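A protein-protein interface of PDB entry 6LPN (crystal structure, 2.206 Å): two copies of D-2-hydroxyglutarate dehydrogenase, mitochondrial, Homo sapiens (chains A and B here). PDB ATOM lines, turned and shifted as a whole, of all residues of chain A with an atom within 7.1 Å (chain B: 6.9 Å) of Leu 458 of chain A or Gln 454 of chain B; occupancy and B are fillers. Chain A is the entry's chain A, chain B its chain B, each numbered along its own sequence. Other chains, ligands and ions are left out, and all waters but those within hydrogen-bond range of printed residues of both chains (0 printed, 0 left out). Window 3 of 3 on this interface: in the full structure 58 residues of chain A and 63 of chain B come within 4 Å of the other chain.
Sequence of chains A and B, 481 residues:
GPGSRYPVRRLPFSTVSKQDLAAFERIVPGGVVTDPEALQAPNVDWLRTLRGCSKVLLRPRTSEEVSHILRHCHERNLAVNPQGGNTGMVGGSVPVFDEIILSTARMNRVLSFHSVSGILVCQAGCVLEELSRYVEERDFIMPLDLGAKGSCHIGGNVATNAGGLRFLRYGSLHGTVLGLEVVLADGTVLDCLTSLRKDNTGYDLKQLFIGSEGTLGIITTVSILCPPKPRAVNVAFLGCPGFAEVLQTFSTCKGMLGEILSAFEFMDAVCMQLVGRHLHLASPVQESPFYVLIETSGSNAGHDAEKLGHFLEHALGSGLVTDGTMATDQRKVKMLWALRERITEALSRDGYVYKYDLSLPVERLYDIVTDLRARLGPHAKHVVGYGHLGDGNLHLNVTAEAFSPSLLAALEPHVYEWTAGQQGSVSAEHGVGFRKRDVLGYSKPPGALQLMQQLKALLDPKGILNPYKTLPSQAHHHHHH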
ATOM      1  N   LEU A 184      -8.348 -20.448 -22.374  1.00  0.00           N
ATOM      2  CA  LEU A 184      -7.188 -19.982 -21.633  1.00  0.00           C
ATOM      3  C   LEU A 184      -7.391 -18.543 -21.171  1.00  0.00           C
ATOM      4  O   LEU A 184      -8.319 -17.850 -21.592  1.00  0.00           O
ATOM      5  CB  LEU A 184      -5.927 -20.099 -22.491  1.00  0.00           C
ATOM      6  CG  LEU A 184      -5.696 -21.511 -23.042  1.00  0.00           C
ATOM      7  CD1 LEU A 184      -4.455 -21.579 -23.918  1.00  0.00           C
ATOM      8  CD2 LEU A 184      -5.596 -22.504 -21.884  1.00  0.00           C
ATOM      9  N   TYR A 203       1.536 -34.691 -27.363  1.00  0.00           N
ATOM     10  CA  TYR A 203       1.409 -34.619 -25.919  1.00  0.00           C
ATOM     11  C   TYR A 203      -0.060 -34.630 -25.519  1.00  0.00           C
ATOM     12  O   TYR A 203      -0.916 -34.076 -26.214  1.00  0.00           O
ATOM     13  CB  TYR A 203       2.069 -33.350 -25.372  1.00  0.00           C
ATOM     14  CG  TYR A 203       3.515 -33.109 -25.764  1.00  0.00           C
ATOM     15  CD1 TYR A 203       4.373 -34.163 -26.081  1.00  0.00           C
ATOM     16  CD2 TYR A 203       4.030 -31.820 -25.777  1.00  0.00           C
ATOM     17  CE1 TYR A 203       5.702 -33.926 -26.418  1.00  0.00           C
ATOM     18  CE2 TYR A 203       5.363 -31.572 -26.108  1.00  0.00           C
ATOM     19  CZ  TYR A 203       6.191 -32.623 -26.428  1.00  0.00           C
ATOM     20  OH  TYR A 203       7.506 -32.359 -26.755  1.00  0.00           O
ATOM     21  N   LEU A 216      -5.310 -22.792 -14.676  1.00  0.00           N
ATOM     22  CA  LEU A 216      -4.668 -22.871 -15.980  1.00  0.00           C
ATOM     23  C   LEU A 216      -5.614 -22.637 -17.147  1.00  0.00           C
ATOM     24  O   LEU A 216      -5.140 -22.457 -18.271  1.00  0.00           O
ATOM     25  CB  LEU A 216      -3.996 -24.243 -16.155  1.00  0.00           C
ATOM     26  CG  LEU A 216      -2.914 -24.623 -15.138  1.00  0.00           C
ATOM     27  CD1 LEU A 216      -2.319 -25.996 -15.444  1.00  0.00           C
ATOM     28  CD2 LEU A 216      -1.824 -23.551 -15.079  1.00  0.00           C
ATOM     29  N   MET A 452       5.457 -26.604 -11.373  1.00  0.00           N
ATOM     30  CA  MET A 452       4.045 -26.222 -11.373  1.00  0.00           C
ATOM     31  C   MET A 452       3.896 -24.718 -11.565  1.00  0.00           C
ATOM     32  O   MET A 452       3.062 -24.252 -12.350  1.00  0.00           O
ATOM     33  CB  MET A 452       3.373 -26.649 -10.066  1.00  0.00           C
ATOM     34  CG  MET A 452       3.312 -28.144  -9.833  1.00  0.00           C
ATOM     35  SD  MET A 452       2.403 -28.543  -8.320  1.00  0.00           S
ATOM     36  CE  MET A 452       2.867 -30.279  -8.131  1.00  0.00           C
ATOM     37  N   GLN A 453       4.690 -23.945 -10.824  1.00  0.00           N
ATOM     38  CA  GLN A 453       4.671 -22.490 -10.958  1.00  0.00           C
ATOM     39  C   GLN A 453       5.098 -22.039 -12.353  1.00  0.00           C
ATOM     40  O   GLN A 453       4.561 -21.054 -12.878  1.00  0.00           O
ATOM     41  CB  GLN A 453       5.560 -21.857  -9.887  1.00  0.00           C
ATOM     42  CG  GLN A 453       5.050 -22.111  -8.473  1.00  0.00           C
ATOM     43  CD  GLN A 453       5.847 -21.385  -7.414  1.00  0.00           C
ATOM     44  OE1 GLN A 453       7.061 -21.207  -7.543  1.00  0.00           O
ATOM     45  NE2 GLN A 453       5.165 -20.952  -6.355  1.00  0.00           N
ATOM     46  N   GLN A 454       6.070 -22.733 -12.966  1.00  0.00           N
ATOM     47  CA  GLN A 454       6.465 -22.404 -14.335  1.00  0.00           C
ATOM     48  C   GLN A 454       5.339 -22.661 -15.334  1.00  0.00           C
ATOM     49  O   GLN A 454       5.145 -21.873 -16.267  1.00  0.00           O
ATOM     50  CB  GLN A 454       7.710 -23.194 -14.742  1.00  0.00           C
ATOM     51  CG  GLN A 454       8.987 -22.870 -13.971  1.00  0.00           C
ATOM     52  CD  GLN A 454      10.137 -23.781 -14.392  1.00  0.00           C
ATOM     53  OE1 GLN A 454      10.494 -24.728 -13.693  1.00  0.00           O
ATOM     54  NE2 GLN A 454      10.716 -23.493 -15.546  1.00  0.00           N
ATOM     55  N   LEU A 455       4.587 -23.750 -15.161  1.00  0.00           N
ATOM     56  CA  LEU A 455       3.451 -23.990 -16.050  1.00  0.00           C
ATOM     57  C   LEU A 455       2.371 -22.930 -15.869  1.00  0.00           C
ATOM     58  O   LEU A 455       1.781 -22.462 -16.850  1.00  0.00           O
ATOM     59  CB  LEU A 455       2.862 -25.384 -15.834  1.00  0.00           C
ATOM     60  CG  LEU A 455       3.701 -26.574 -16.296  1.00  0.00           C
ATOM     61  CD1 LEU A 455       3.151 -27.841 -15.679  1.00  0.00           C
ATOM     62  CD2 LEU A 455       3.733 -26.674 -17.821  1.00  0.00           C
ATOM     63  N   LYS A 456       2.080 -22.563 -14.616  1.00  0.00           N
ATOM     64  CA  LYS A 456       1.148 -21.474 -14.346  1.00  0.00           C
ATOM     65  C   LYS A 456       1.572 -20.184 -15.043  1.00  0.00           C
ATOM     66  O   LYS A 456       0.745 -19.507 -15.664  1.00  0.00           O
ATOM     67  CB  LYS A 456       1.040 -21.265 -12.828  1.00  0.00           C
ATOM     68  CG  LYS A 456       0.239 -20.039 -12.365  1.00  0.00           C
ATOM     69  CD  LYS A 456      -1.188 -20.040 -12.887  1.00  0.00           C
ATOM     70  CE  LYS A 456      -1.918 -18.777 -12.437  1.00  0.00           C
ATOM     71  NZ  LYS A 456      -3.396 -18.868 -12.648  1.00  0.00           N
ATOM     72  N   ALA A 457       2.863 -19.849 -14.980  1.00  0.00           N
ATOM     73  CA  ALA A 457       3.384 -18.641 -15.617  1.00  0.00           C
ATOM     74  C   ALA A 457       3.289 -18.702 -17.140  1.00  0.00           C
ATOM     75  O   ALA A 457       3.068 -17.671 -17.785  1.00  0.00           O
ATOM     76  CB  ALA A 457       4.832 -18.413 -15.183  1.00  0.00           C
ATOM     77  N   LEU A 458       3.460 -19.891 -17.727  1.00  0.00           N
ATOM     78  CA  LEU A 458       3.301 -20.056 -19.170  1.00  0.00           C
ATOM     79  C   LEU A 458       1.846 -19.886 -19.612  1.00  0.00           C
ATOM     80  O   LEU A 458       1.565 -19.163 -20.576  1.00  0.00           O
ATOM     81  CB  LEU A 458       3.819 -21.438 -19.579  1.00  0.00           C
ATOM     82  CG  LEU A 458       3.552 -21.905 -21.015  1.00  0.00           C
ATOM     83  CD1 LEU A 458       4.116 -20.916 -22.037  1.00  0.00           C
ATOM     84  CD2 LEU A 458       4.065 -23.327 -21.260  1.00  0.00           C
ATOM     85  N   LEU A 459       0.904 -20.538 -18.922  1.00  0.00           N
ATOM     86  CA  LEU A 459      -0.489 -20.543 -19.379  1.00  0.00           C
ATOM     87  C   LEU A 459      -1.260 -19.292 -18.971  1.00  0.00           C
ATOM     88  O   LEU A 459      -2.237 -18.938 -19.638  1.00  0.00           O
ATOM     89  CB  LEU A 459      -1.223 -21.796 -18.900  1.00  0.00           C
ATOM     90  CG  LEU A 459      -0.776 -23.040 -19.664  1.00  0.00           C
ATOM     91  CD1 LEU A 459      -1.270 -24.292 -18.972  1.00  0.00           C
ATOM     92  CD2 LEU A 459      -1.251 -22.982 -21.124  1.00  0.00           C
ATOM     93  N   ASP A 460      -0.880 -18.648 -17.866  1.00  0.00           N
ATOM     94  CA  ASP A 460      -1.601 -17.483 -17.340  1.00  0.00           C
ATOM     95  C   ASP A 460      -0.575 -16.542 -16.717  1.00  0.00           C
ATOM     96  O   ASP A 460      -0.490 -16.398 -15.491  1.00  0.00           O
ATOM     97  CB  ASP A 460      -2.666 -17.915 -16.329  1.00  0.00           C
ATOM     98  CG  ASP A 460      -3.380 -16.734 -15.651  1.00  0.00           C
ATOM     99  OD1 ASP A 460      -3.429 -15.620 -16.219  1.00  0.00           O
ATOM    100  OD2 ASP A 460      -3.905 -16.932 -14.536  1.00  0.00           O
ATOM    101  N   PRO A 461       0.240 -15.885 -17.553  1.00  0.00           N
ATOM    102  CA  PRO A 461       1.306 -15.007 -17.024  1.00  0.00           C
ATOM    103  C   PRO A 461       0.813 -13.865 -16.146  1.00  0.00           C
ATOM    104  O   PRO A 461       1.504 -13.484 -15.190  1.00  0.00           O
ATOM    105  CB  PRO A 461       1.977 -14.464 -18.299  1.00  0.00           C
ATOM    106  CG  PRO A 461       0.976 -14.712 -19.419  1.00  0.00           C
ATOM    107  CD  PRO A 461       0.251 -15.957 -19.025  1.00  0.00           C
ATOM    108  N   GLY B 447      -3.802 -24.771 -32.852  1.00  0.00           N
ATOM    109  CA  GLY B 447      -3.614 -24.204 -31.522  1.00  0.00           C
ATOM    110  C   GLY B 447      -3.110 -25.207 -30.500  1.00  0.00           C
ATOM    111  O   GLY B 447      -2.317 -24.863 -29.621  1.00  0.00           O
ATOM    112  N   LEU B 449      -1.235 -27.861 -31.285  1.00  0.00           N
ATOM    113  CA  LEU B 449       0.156 -28.079 -31.679  1.00  0.00           C
ATOM    114  C   LEU B 449       1.074 -26.963 -31.195  1.00  0.00           C
ATOM    115  O   LEU B 449       2.209 -27.231 -30.792  1.00  0.00           O
ATOM    116  CB  LEU B 449       0.252 -28.235 -33.199  1.00  0.00           C
ATOM    117  CG  LEU B 449      -0.488 -29.451 -33.769  1.00  0.00           C
ATOM    118  CD1 LEU B 449      -0.419 -29.492 -35.290  1.00  0.00           C
ATOM    119  CD2 LEU B 449       0.067 -30.748 -33.177  1.00  0.00           C
ATOM    120  N   GLN B 450       0.585 -25.721 -31.165  1.00  0.00           N
ATOM    121  CA  GLN B 450       1.420 -24.629 -30.677  1.00  0.00           C
ATOM    122  C   GLN B 450       1.684 -24.764 -29.178  1.00  0.00           C
ATOM    123  O   GLN B 450       2.816 -24.547 -28.728  1.00  0.00           O
ATOM    124  CB  GLN B 450       0.770 -23.284 -31.013  1.00  0.00           C
ATOM    125  CG  GLN B 450       1.624 -22.069 -30.679  1.00  0.00           C
ATOM    126  CD  GLN B 450       0.836 -20.776 -30.730  1.00  0.00           C
ATOM    127  OE1 GLN B 450       0.620 -20.202 -31.803  1.00  0.00           O
ATOM    128  NE2 GLN B 450       0.400 -20.307 -29.570  1.00  0.00           N
ATOM    129  N   LEU B 451       0.656 -25.084 -28.384  1.00  0.00           N
ATOM    130  CA  LEU B 451       0.878 -25.254 -26.949  1.00  0.00           C
ATOM    131  C   LEU B 451       1.897 -26.357 -26.672  1.00  0.00           C
ATOM    132  O   LEU B 451       2.691 -26.255 -25.730  1.00  0.00           O
ATOM    133  CB  LEU B 451      -0.441 -25.543 -26.238  1.00  0.00           C
ATOM    134  CG  LEU B 451      -0.346 -25.800 -24.736  1.00  0.00           C
ATOM    135  CD1 LEU B 451       0.320 -24.621 -24.042  1.00  0.00           C
ATOM    136  CD2 LEU B 451      -1.754 -26.002 -24.180  1.00  0.00           C
ATOM    137  N   MET B 452       1.886 -27.421 -27.480  1.00  0.00           N
ATOM    138  CA  MET B 452       2.910 -28.456 -27.364  1.00  0.00           C
ATOM    139  C   MET B 452       4.306 -27.895 -27.626  1.00  0.00           C
ATOM    140  O   MET B 452       5.266 -28.268 -26.944  1.00  0.00           O
ATOM    141  CB  MET B 452       2.653 -29.615 -28.331  1.00  0.00           C
ATOM    142  CG  MET B 452       1.431 -30.470 -28.048  1.00  0.00           C
ATOM    143  SD  MET B 452       1.169 -31.639 -29.404  1.00  0.00           S
ATOM    144  CE  MET B 452      -0.566 -32.056 -29.145  1.00  0.00           C
ATOM    145  N   GLN B 453       4.432 -27.009 -28.618  1.00  0.00           N
ATOM    146  CA  GLN B 453       5.719 -26.398 -28.935  1.00  0.00           C
ATOM    147  C   GLN B 453       6.218 -25.549 -27.768  1.00  0.00           C
ATOM    148  O   GLN B 453       7.403 -25.590 -27.417  1.00  0.00           O
ATOM    149  CB  GLN B 453       5.524 -25.480 -30.144  1.00  0.00           C
ATOM    150  CG  GLN B 453       5.025 -26.104 -31.458  1.00  0.00           C
ATOM    151  CD  GLN B 453       6.083 -26.625 -32.400  1.00  0.00           C
ATOM    152  OE1 GLN B 453       7.242 -26.806 -32.025  1.00  0.00           O
ATOM    153  NE2 GLN B 453       5.689 -26.842 -33.657  1.00  0.00           N
ATOM    154  N   GLN B 454       5.304 -24.825 -27.119  1.00  0.00           N
ATOM    155  CA  GLN B 454       5.631 -24.028 -25.941  1.00  0.00           C
ATOM    156  C   GLN B 454       6.038 -24.901 -24.764  1.00  0.00           C
ATOM    157  O   GLN B 454       6.937 -24.535 -23.998  1.00  0.00           O
ATOM    158  CB  GLN B 454       4.441 -23.156 -25.551  1.00  0.00           C
ATOM    159  CG  GLN B 454       4.075 -22.079 -26.554  1.00  0.00           C
ATOM    160  CD  GLN B 454       2.755 -21.414 -26.204  1.00  0.00           C
ATOM    161  OE1 GLN B 454       1.714 -21.745 -26.772  1.00  0.00           O
ATOM    162  NE2 GLN B 454       2.782 -20.507 -25.233  1.00  0.00           N
ATOM    163  N   LEU B 455       5.376 -26.045 -24.588  1.00  0.00           N
ATOM    164  CA  LEU B 455       5.797 -26.970 -23.541  1.00  0.00           C
ATOM    165  C   LEU B 455       7.225 -27.441 -23.769  1.00  0.00           C
ATOM    166  O   LEU B 455       8.025 -27.505 -22.827  1.00  0.00           O
ATOM    167  CB  LEU B 455       4.844 -28.164 -23.457  1.00  0.00           C
ATOM    168  CG  LEU B 455       3.443 -27.920 -22.878  1.00  0.00           C
ATOM    169  CD1 LEU B 455       2.643 -29.212 -22.890  1.00  0.00           C
ATOM    170  CD2 LEU B 455       3.501 -27.322 -21.475  1.00  0.00           C
ATOM    171  N   LYS B 456       7.547 -27.804 -25.011  1.00  0.00           N
ATOM    172  CA  LYS B 456       8.901 -28.220 -25.374  1.00  0.00           C
ATOM    173  C   LYS B 456       9.927 -27.122 -25.099  1.00  0.00           C
ATOM    174  O   LYS B 456      10.992 -27.383 -24.527  1.00  0.00           O
ATOM    175  CB  LYS B 456       8.919 -28.627 -26.853  1.00  0.00           C
ATOM    176  CG  LYS B 456      10.287 -28.991 -27.456  1.00  0.00           C
ATOM    177  CD  LYS B 456      10.932 -30.206 -26.796  1.00  0.00           C
ATOM    178  CE  LYS B 456      12.318 -30.484 -27.397  1.00  0.00           C
ATOM    179  NZ  LYS B 456      12.946 -31.771 -26.916  1.00  0.00           N
ATOM    180  N   ALA B 457       9.622 -25.882 -25.510  1.00  0.00           N
ATOM    181  CA  ALA B 457      10.532 -24.755 -25.282  1.00  0.00           C
ATOM    182  C   ALA B 457      10.755 -24.490 -23.799  1.00  0.00           C
ATOM    183  O   ALA B 457      11.879 -24.193 -23.375  1.00  0.00           O
ATOM    184  CB  ALA B 457       9.998 -23.495 -25.966  1.00  0.00           C
ATOM    185  N   LEU B 458       9.695 -24.589 -22.995  1.00  0.00           N
ATOM    186  CA  LEU B 458       9.836 -24.448 -21.549  1.00  0.00           C
ATOM    187  C   LEU B 458      10.719 -25.539 -20.966  1.00  0.00           C
ATOM    188  O   LEU B 458      11.604 -25.266 -20.147  1.00  0.00           O
ATOM    189  CB  LEU B 458       8.459 -24.478 -20.881  1.00  0.00           C
ATOM    190  CG  LEU B 458       8.431 -24.419 -19.346  1.00  0.00           C
ATOM    191  CD1 LEU B 458       8.892 -23.079 -18.798  1.00  0.00           C
ATOM    192  CD2 LEU B 458       7.049 -24.753 -18.840  1.00  0.00           C
ATOM    193  N   LEU B 459      10.478 -26.788 -21.347  1.00  0.00           N
ATOM    194  CA  LEU B 459      11.154 -27.890 -20.674  1.00  0.00           C
ATOM    195  C   LEU B 459      12.515 -28.224 -21.278  1.00  0.00           C
ATOM    196  O   LEU B 459      13.407 -28.671 -20.552  1.00  0.00           O
ATOM    197  CB  LEU B 459      10.251 -29.123 -20.676  1.00  0.00           C
ATOM    198  CG  LEU B 459       9.122 -29.024 -19.647  1.00  0.00           C
ATOM    199  CD1 LEU B 459       8.065 -30.041 -19.968  1.00  0.00           C
ATOM    200  CD2 LEU B 459       9.630 -29.180 -18.215  1.00  0.00           C
ATOM    201  N   ASP B 460      12.712 -27.987 -22.574  1.00  0.00           N
ATOM    202  CA  ASP B 460      13.981 -28.269 -23.255  1.00  0.00           C
ATOM    203  C   ASP B 460      14.271 -27.139 -24.239  1.00  0.00           C
ATOM    204  O   ASP B 460      14.193 -27.317 -25.461  1.00  0.00           O
ATOM    205  CB  ASP B 460      13.903 -29.628 -23.965  1.00  0.00           C
ATOM    206  CG  ASP B 460      15.208 -30.017 -24.700  1.00  0.00           C
ATOM    207  OD1 ASP B 460      16.290 -29.442 -24.422  1.00  0.00           O
ATOM    208  OD2 ASP B 460      15.134 -30.904 -25.583  1.00  0.00           O
ATOM    209  N   LEU B 471       7.129 -33.483 -32.396  1.00  0.00           N
ATOM    210  CA  LEU B 471       6.361 -32.330 -32.854  1.00  0.00           C
ATOM    211  C   LEU B 471       6.706 -31.965 -34.297  1.00  0.00           C
ATOM    212  O   LEU B 471       7.776 -32.322 -34.795  1.00  0.00           O
ATOM    213  CB  LEU B 471       6.621 -31.135 -31.932  1.00  0.00           C
ATOM    214  CG  LEU B 471       6.455 -31.416 -30.443  1.00  0.00           C
ATOM    215  CD1 LEU B 471       6.938 -30.225 -29.628  1.00  0.00           C
ATOM    216  CD2 LEU B 471       4.986 -31.728 -30.145  1.00  0.00           C
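Among the printed residues, pairs that only touch across the chains: Tyr 203 of chain A with Lys 456 of chain B (3.99 Å), Tyr 203 of chain A with Leu 471 of chain B (3.6 Å), Gln 454 of chain A with Leu 458 of chain B (3.8 Å), Leu 455 of chain A with Leu 455 of chain B (3.7 Å), Leu 455 of chain A with Leu 458 of chain B (3.97 Å), Leu 458 of chain A with Gln 454 of chain B (3.5 Å) and Leu 459 of chain A with Leu 451 of chain B (3.7 Å).
NE2 of Gln 450 of chain B sits at hydrogen-bond distance from OE1 of Gln 454 of chain B (3.4 Å).
The side-chain amino group (NZ) of Lys 456 of chain B lies within salt-bridge range of the side-chain carboxylate (OD2) of Asp 460 of chain B (2.7 Å).
N of Tyr 203 of chain A is in hydrogen-bond range of SD of Met 452 of chain B, at 3.7 Å.
Gln 454 of chain A touches Leu 458 of chain B, and with the chains exchanged Leu 458 of chain A touches Gln 454 of chain B.
Leu 455 of chain A touches its own counterpart, Leu 455 of chain B.
Leu 455 of chain A touches Leu 458 of chain B, but with the chains exchanged Leu 458 of chain A does not touch Leu 455 of chain B (4.04 Å).
9 positions are printed for both chains.
Of the printed residues of chain B, Tyr 203 of chain A touches Met 452, Lys 456 and Leu 471.
Leu 458 of chain A touches one residue of chain B.
Of chain A, only Leu 458 comes within 4 Å of Gln 454 of chain B.
Printed residues of chain A within 4 Å of Leu 471 of chain B: Tyr 203 (3.6 Å).
The nearest printed residue of chain A that does not touch Leu 451 of chain B is Leu 458 of chain A (4.8 Å).
Of the 13 printed residues of chain A, 5 touch a printed residue of chain B.
Along chain A the printed residues that touch a printed residue of chain B span positions 203 to 459.
Of the 14 printed residues of chain B, 7 touch a printed residue of chain A.
Hydrophobic or aromatic side chains of chain B that line the printed part of chain A: Leu 451, Met 452, Leu 455, Leu 458 and Leu 471.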
